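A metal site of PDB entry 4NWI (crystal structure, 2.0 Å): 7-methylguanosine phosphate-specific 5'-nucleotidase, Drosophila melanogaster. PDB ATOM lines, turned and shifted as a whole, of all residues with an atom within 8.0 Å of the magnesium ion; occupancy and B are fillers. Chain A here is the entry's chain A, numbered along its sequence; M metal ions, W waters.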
ATOM      1  N   SER A  54      31.388   6.582 -18.817  1.00  0.00           N
ATOM      2  CA  SER A  54      29.939   6.599 -18.976  1.00  0.00           C
ATOM      3  C   SER A  54      29.186   6.664 -17.651  1.00  0.00           C
ATOM      4  O   SER A  54      29.567   6.019 -16.666  1.00  0.00           O
ATOM      5  CB  SER A  54      29.470   5.390 -19.792  1.00  0.00           C
ATOM      6  OG  SER A  54      28.057   5.383 -19.936  1.00  0.00           O
ATOM      7  N   ASP A  55      28.123   7.455 -17.627  1.00  0.00           N
ATOM      8  CA  ASP A  55      27.182   7.477 -16.512  1.00  0.00           C
ATOM      9  C   ASP A  55      26.425   6.155 -16.567  1.00  0.00           C
ATOM     10  O   ASP A  55      26.426   5.478 -17.595  1.00  0.00           O
ATOM     11  CB  ASP A  55      26.218   8.659 -16.682  1.00  0.00           C
ATOM     12  CG  ASP A  55      25.090   8.642 -15.677  1.00  0.00           C
ATOM     13  OD1 ASP A  55      25.370   8.589 -14.459  1.00  0.00           O
ATOM     14  OD2 ASP A  55      23.921   8.666 -16.111  1.00  0.00           O
ATOM     15  N   PHE A  56      25.787   5.767 -15.465  1.00  0.00           N
ATOM     16  CA  PHE A  56      24.992   4.540 -15.474  1.00  0.00           C
ATOM     17  C   PHE A  56      23.505   4.812 -15.656  1.00  0.00           C
ATOM     18  O   PHE A  56      22.930   4.483 -16.700  1.00  0.00           O
ATOM     19  CB  PHE A  56      25.231   3.709 -14.206  1.00  0.00           C
ATOM     20  CG  PHE A  56      24.323   2.512 -14.107  1.00  0.00           C
ATOM     21  CD1 PHE A  56      24.515   1.401 -14.905  1.00  0.00           C
ATOM     22  CD2 PHE A  56      23.246   2.523 -13.219  1.00  0.00           C
ATOM     23  CE1 PHE A  56      23.673   0.309 -14.819  1.00  0.00           C
ATOM     24  CE2 PHE A  56      22.394   1.430 -13.143  1.00  0.00           C
ATOM     25  CZ  PHE A  56      22.616   0.322 -13.942  1.00  0.00           C
ATOM     26  N   ASP A  57      22.893   5.395 -14.627  1.00  0.00           N
ATOM     27  CA  ASP A  57      21.443   5.539 -14.586  1.00  0.00           C
ATOM     28  C   ASP A  57      20.867   6.362 -15.734  1.00  0.00           C
ATOM     29  O   ASP A  57      21.125   7.562 -15.847  1.00  0.00           O
ATOM     30  CB  ASP A  57      21.008   6.118 -13.229  1.00  0.00           C
ATOM     31  CG  ASP A  57      21.187   5.138 -12.097  1.00  0.00           C
ATOM     32  OD1 ASP A  57      20.457   4.129 -12.061  1.00  0.00           O
ATOM     33  OD2 ASP A  57      22.069   5.364 -11.238  1.00  0.00           O
ATOM     34  N   TYR A  58      20.089   5.682 -16.568  1.00  0.00           N
ATOM     35  CA  TYR A  58      19.385   6.271 -17.703  1.00  0.00           C
ATOM     36  C   TYR A  58      20.337   6.739 -18.801  1.00  0.00           C
ATOM     37  O   TYR A  58      19.978   7.535 -19.673  1.00  0.00           O
ATOM     38  CB  TYR A  58      18.438   7.375 -17.230  1.00  0.00           C
ATOM     39  CG  TYR A  58      17.599   6.895 -16.076  1.00  0.00           C
ATOM     40  CD1 TYR A  58      16.631   5.928 -16.254  1.00  0.00           C
ATOM     41  CD2 TYR A  58      17.808   7.395 -14.799  1.00  0.00           C
ATOM     42  CE1 TYR A  58      15.874   5.467 -15.199  1.00  0.00           C
ATOM     43  CE2 TYR A  58      17.051   6.944 -13.733  1.00  0.00           C
ATOM     44  CZ  TYR A  58      16.095   5.983 -13.945  1.00  0.00           C
ATOM     45  OH  TYR A  58      15.341   5.536 -12.892  1.00  0.00           O
ATOM     46  N   THR A  59      21.545   6.196 -18.754  1.00  0.00           N
ATOM     47  CA  THR A  59      22.484   6.271 -19.861  1.00  0.00           C
ATOM     48  C   THR A  59      22.730   4.855 -20.361  1.00  0.00           C
ATOM     49  O   THR A  59      22.550   4.560 -21.536  1.00  0.00           O
ATOM     50  CB  THR A  59      23.822   6.898 -19.440  1.00  0.00           C
ATOM     51  OG1 THR A  59      23.624   8.289 -19.142  1.00  0.00           O
ATOM     52  CG2 THR A  59      24.841   6.769 -20.559  1.00  0.00           C
ATOM     53  N   ILE A  60      23.138   3.981 -19.445  1.00  0.00           N
ATOM     54  CA  ILE A  60      23.299   2.557 -19.753  1.00  0.00           C
ATOM     55  C   ILE A  60      21.937   1.859 -19.672  1.00  0.00           C
ATOM     56  O   ILE A  60      21.599   1.033 -20.520  1.00  0.00           O
ATOM     57  CB  ILE A  60      24.339   1.879 -18.823  1.00  0.00           C
ATOM     58  CG1 ILE A  60      25.748   2.358 -19.169  1.00  0.00           C
ATOM     59  CG2 ILE A  60      24.258   0.369 -18.934  1.00  0.00           C
ATOM     60  CD1 ILE A  60      26.833   1.802 -18.251  1.00  0.00           C
ATOM     61  N   THR A  61      21.143   2.211 -18.656  1.00  0.00           N
ATOM     62  CA  THR A  61      19.745   1.807 -18.623  1.00  0.00           C
ATOM     63  C   THR A  61      18.909   2.759 -19.493  1.00  0.00           C
ATOM     64  O   THR A  61      19.377   3.834 -19.862  1.00  0.00           O
ATOM     65  CB  THR A  61      19.169   1.776 -17.182  1.00  0.00           C
ATOM     66  OG1 THR A  61      19.496   2.991 -16.505  1.00  0.00           O
ATOM     67  CG2 THR A  61      19.736   0.595 -16.409  1.00  0.00           C
ATOM     68  N   GLN A  63      15.956   5.372 -20.718  1.00  0.00           N
ATOM     69  CA  GLN A  63      15.102   6.454 -20.249  1.00  0.00           C
ATOM     70  C   GLN A  63      13.677   6.135 -20.685  1.00  0.00           C
ATOM     71  O   GLN A  63      12.709   6.427 -19.987  1.00  0.00           O
ATOM     72  CB  GLN A  63      15.555   7.797 -20.821  1.00  0.00           C
ATOM     73  CG  GLN A  63      17.022   7.829 -21.248  1.00  0.00           C
ATOM     74  CD  GLN A  63      17.490   9.208 -21.663  1.00  0.00           C
ATOM     75  OE1 GLN A  63      17.456   9.558 -22.856  1.00  0.00           O
ATOM     76  NE2 GLN A  63      17.935   9.998 -20.699  1.00  0.00           N
ATOM     77  N   PHE A 170      31.090   5.732 -14.258  1.00  0.00           N
ATOM     78  CA  PHE A 170      31.218   6.743 -13.218  1.00  0.00           C
ATOM     79  C   PHE A 170      29.815   7.083 -12.741  1.00  0.00           C
ATOM     80  O   PHE A 170      29.035   7.691 -13.469  1.00  0.00           O
ATOM     81  CB  PHE A 170      31.893   7.977 -13.812  1.00  0.00           C
ATOM     82  CG  PHE A 170      32.504   8.907 -12.794  1.00  0.00           C
ATOM     83  CD1 PHE A 170      32.103   8.864 -11.465  1.00  0.00           C
ATOM     84  CD2 PHE A 170      33.468   9.828 -13.175  1.00  0.00           C
ATOM     85  CE1 PHE A 170      32.672   9.717 -10.532  1.00  0.00           C
ATOM     86  CE2 PHE A 170      34.033  10.688 -12.249  1.00  0.00           C
ATOM     87  CZ  PHE A 170      33.637  10.629 -10.924  1.00  0.00           C
ATOM     88  N   SER A 171      29.485   6.690 -11.512  1.00  0.00           N
ATOM     89  CA  SER A 171      28.109   6.852 -11.035  1.00  0.00           C
ATOM     90  C   SER A 171      28.017   7.396  -9.606  1.00  0.00           C
ATOM     91  O   SER A 171      28.763   6.978  -8.718  1.00  0.00           O
ATOM     92  CB  SER A 171      27.363   5.513 -11.131  1.00  0.00           C
ATOM     93  OG  SER A 171      26.054   5.617 -10.599  1.00  0.00           O
ATOM     94  N   ALA A 172      27.100   8.325  -9.403  1.00  0.00           N
ATOM     95  CA  ALA A 172      26.834   8.869  -8.070  1.00  0.00           C
ATOM     96  C   ALA A 172      25.759   8.041  -7.370  1.00  0.00           C
ATOM     97  O   ALA A 172      25.221   8.447  -6.338  1.00  0.00           O
ATOM     98  CB  ALA A 172      26.425  10.327  -8.170  1.00  0.00           C
ATOM     99  N   THR A 216      26.015  13.924  -7.290  1.00  0.00           N
ATOM    100  CA  THR A 216      25.772  14.348  -8.668  1.00  0.00           C
ATOM    101  C   THR A 216      26.634  15.560  -9.089  1.00  0.00           C
ATOM    102  O   THR A 216      26.831  15.812 -10.285  1.00  0.00           O
ATOM    103  CB  THR A 216      24.252  14.563  -8.905  1.00  0.00           C
ATOM    104  OG1 THR A 216      23.578  13.302  -8.886  1.00  0.00           O
ATOM    105  CG2 THR A 216      23.959  15.245 -10.232  1.00  0.00           C
ATOM    106  N   LYS A 219      31.059  14.500  -9.869  1.00  0.00           N
ATOM    107  CA  LYS A 219      31.392  13.486 -10.850  1.00  0.00           C
ATOM    108  C   LYS A 219      32.367  14.127 -11.827  1.00  0.00           C
ATOM    109  O   LYS A 219      32.036  14.414 -12.971  1.00  0.00           O
ATOM    110  CB  LYS A 219      30.144  13.053 -11.622  1.00  0.00           C
ATOM    111  CG  LYS A 219      29.251  12.067 -10.891  1.00  0.00           C
ATOM    112  CD  LYS A 219      28.030  11.718 -11.736  1.00  0.00           C
ATOM    113  CE  LYS A 219      28.407  10.936 -12.981  1.00  0.00           C
ATOM    114  NZ  LYS A 219      27.307  10.080 -13.467  1.00  0.00           N
ATOM    115  N   MET A 243      29.857   9.746 -21.958  1.00  0.00           N
ATOM    116  CA  MET A 243      28.447   9.498 -22.248  1.00  0.00           C
ATOM    117  C   MET A 243      27.564   9.771 -21.032  1.00  0.00           C
ATOM    118  O   MET A 243      27.834   9.271 -19.947  1.00  0.00           O
ATOM    119  CB  MET A 243      28.246   8.062 -22.729  1.00  0.00           C
ATOM    120  CG  MET A 243      28.939   7.746 -24.041  1.00  0.00           C
ATOM    121  SD  MET A 243      29.008   5.980 -24.380  1.00  0.00           S
ATOM    122  CE  MET A 243      27.268   5.550 -24.211  1.00  0.00           C
ATOM    123  N   GLY A 244      26.510  10.557 -21.212  1.00  0.00           N
ATOM    124  CA  GLY A 244      25.623  10.855 -20.096  1.00  0.00           C
ATOM    125  C   GLY A 244      24.265  11.392 -20.499  1.00  0.00           C
ATOM    126  O   GLY A 244      24.089  11.820 -21.628  1.00  0.00           O
ATOM    127  N   ASP A 245      23.315  11.386 -19.569  1.00  0.00           N
ATOM    128  CA  ASP A 245      21.973  11.889 -19.875  1.00  0.00           C
ATOM    129  C   ASP A 245      21.681  13.170 -19.102  1.00  0.00           C
ATOM    130  O   ASP A 245      20.585  13.743 -19.208  1.00  0.00           O
ATOM    131  CB  ASP A 245      20.917  10.829 -19.564  1.00  0.00           C
ATOM    132  CG  ASP A 245      20.827  10.516 -18.087  1.00  0.00           C
ATOM    133  OD1 ASP A 245      21.876  10.211 -17.473  1.00  0.00           O
ATOM    134  OD2 ASP A 245      19.714  10.568 -17.533  1.00  0.00           O
ATOM    135  N   SER A 246      22.657  13.616 -18.312  1.00  0.00           N
ATOM    136  CA  SER A 246      22.527  14.837 -17.534  1.00  0.00           C
ATOM    137  C   SER A 246      23.662  15.773 -17.870  1.00  0.00           C
ATOM    138  O   SER A 246      24.715  15.343 -18.353  1.00  0.00           O
ATOM    139  CB  SER A 246      22.533  14.506 -16.044  1.00  0.00           C
ATOM    140  OG  SER A 246      21.544  13.548 -15.717  1.00  0.00           O
ATOM    141  N   ILE A 247      23.455  17.068 -17.620  1.00  0.00           N
ATOM    142  CA  ILE A 247      24.460  18.075 -17.905  1.00  0.00           C
ATOM    143  C   ILE A 247      25.764  17.810 -17.159  1.00  0.00           C
ATOM    144  O   ILE A 247      26.851  17.852 -17.741  1.00  0.00           O
ATOM    145  CB  ILE A 247      23.946  19.491 -17.563  1.00  0.00           C
ATOM    146  CG1 ILE A 247      22.881  19.923 -18.578  1.00  0.00           C
ATOM    147  CG2 ILE A 247      25.091  20.486 -17.553  1.00  0.00           C
ATOM    148  CD1 ILE A 247      23.386  19.967 -20.007  1.00  0.00           C
ATOM    149  N   ASP A 249      27.090  15.085 -16.178  1.00  0.00           N
ATOM    150  CA  ASP A 249      27.815  13.982 -16.808  1.00  0.00           C
ATOM    151  C   ASP A 249      28.853  14.456 -17.811  1.00  0.00           C
ATOM    152  O   ASP A 249      29.848  13.781 -18.068  1.00  0.00           O
ATOM    153  CB  ASP A 249      26.835  13.035 -17.519  1.00  0.00           C
ATOM    154  CG  ASP A 249      25.861  12.365 -16.574  1.00  0.00           C
ATOM    155  OD1 ASP A 249      26.231  12.144 -15.400  1.00  0.00           O
ATOM    156  OD2 ASP A 249      24.738  12.054 -17.009  1.00  0.00           O
ATOM    157  N   MET A 252      32.600  14.608 -16.495  1.00  0.00           N
ATOM    158  CA  MET A 252      33.148  13.434 -15.814  1.00  0.00           C
ATOM    159  C   MET A 252      34.639  13.216 -16.090  1.00  0.00           C
ATOM    160  O   MET A 252      35.355  12.677 -15.247  1.00  0.00           O
ATOM    161  CB  MET A 252      32.360  12.179 -16.179  1.00  0.00           C
ATOM    162  CG  MET A 252      30.986  12.084 -15.528  1.00  0.00           C
ATOM    163  SD  MET A 252      30.136  10.541 -15.884  1.00  0.00           S
ATOM    164  CE  MET A 252      30.075  10.587 -17.673  1.00  0.00           C
ATOM    165  N   PHE A 267      22.415  12.104 -23.938  1.00  0.00           N
ATOM    166  CA  PHE A 267      21.118  11.546 -24.313  1.00  0.00           C
ATOM    167  C   PHE A 267      19.991  12.365 -23.718  1.00  0.00           C
ATOM    168  O   PHE A 267      19.773  12.376 -22.502  1.00  0.00           O
ATOM    169  CB  PHE A 267      21.017  10.094 -23.850  1.00  0.00           C
ATOM    170  CG  PHE A 267      21.984   9.178 -24.538  1.00  0.00           C
ATOM    171  CD1 PHE A 267      21.634   8.556 -25.723  1.00  0.00           C
ATOM    172  CD2 PHE A 267      23.241   8.930 -24.001  1.00  0.00           C
ATOM    173  CE1 PHE A 267      22.519   7.704 -26.369  1.00  0.00           C
ATOM    174  CE2 PHE A 267      24.125   8.087 -24.636  1.00  0.00           C
ATOM    175  CZ  PHE A 267      23.764   7.474 -25.821  1.00  0.00           C
HETATM  176 MG    MG M   1      22.251   9.466 -15.561  1.00  0.00          MG
HETATM  177  O   HOH W   1      22.740   8.995 -13.659  1.00  0.00           O
HETATM  178  O   HOH W   2      20.525  10.340 -14.975  1.00  0.00           O
HETATM  179  O   HOH W   3      23.028  11.305 -15.274  1.00  0.00           O
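The magnesium ion is bound by OD2 of Asp 55 (1.9 Å), water W3 (2.0 Å), water W1 (2.0 Å), water W2 (2.0 Å), OD1 of Asp 245 (2.1 Å) and O of Asp 57 (2.2 Å).
Water W3 bridges the side-chain carboxylate of Asp 249 (2.5 Å) and the side-chain hydroxyl of Ser 246 (2.7 Å). Water W2 bridges the side-chain carboxylate (OD2) of Asp 245 and the side-chain hydroxyl (OG) of Ser 246.
The side-chain carboxylate of Asp 55 lies close to the side-chain hydroxyl of Thr 59. The side-chain carboxylate (OD1) of Asp 55 lies within salt-bridge range of the side-chain amino group (NZ) of Lys 219 (2.6 Å). N of Asp 55 is in hydrogen-bond range of O of Met 243 (3.0 Å). N of Asp 245 sits at hydrogen-bond distance from OD2 of Asp 249 (3.0 Å). The backbone NH (N) of Asp 245 is in hydrogen-bond range of the side-chain hydroxyl (OG1) of Thr 59 (3.1 Å). OD2 of Asp 249 sits at hydrogen-bond distance from N of Ser 246. The side-chain carboxylate of Asp 249 is in salt-bridge range of the side-chain amino group of Lys 219, 3.0 Å away.
OD2 of Asp 249 touches the magnesium ion, at 3.9 Å. Along chain A the residues within 4 Å of the magnesium ion span positions 55 to 249.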
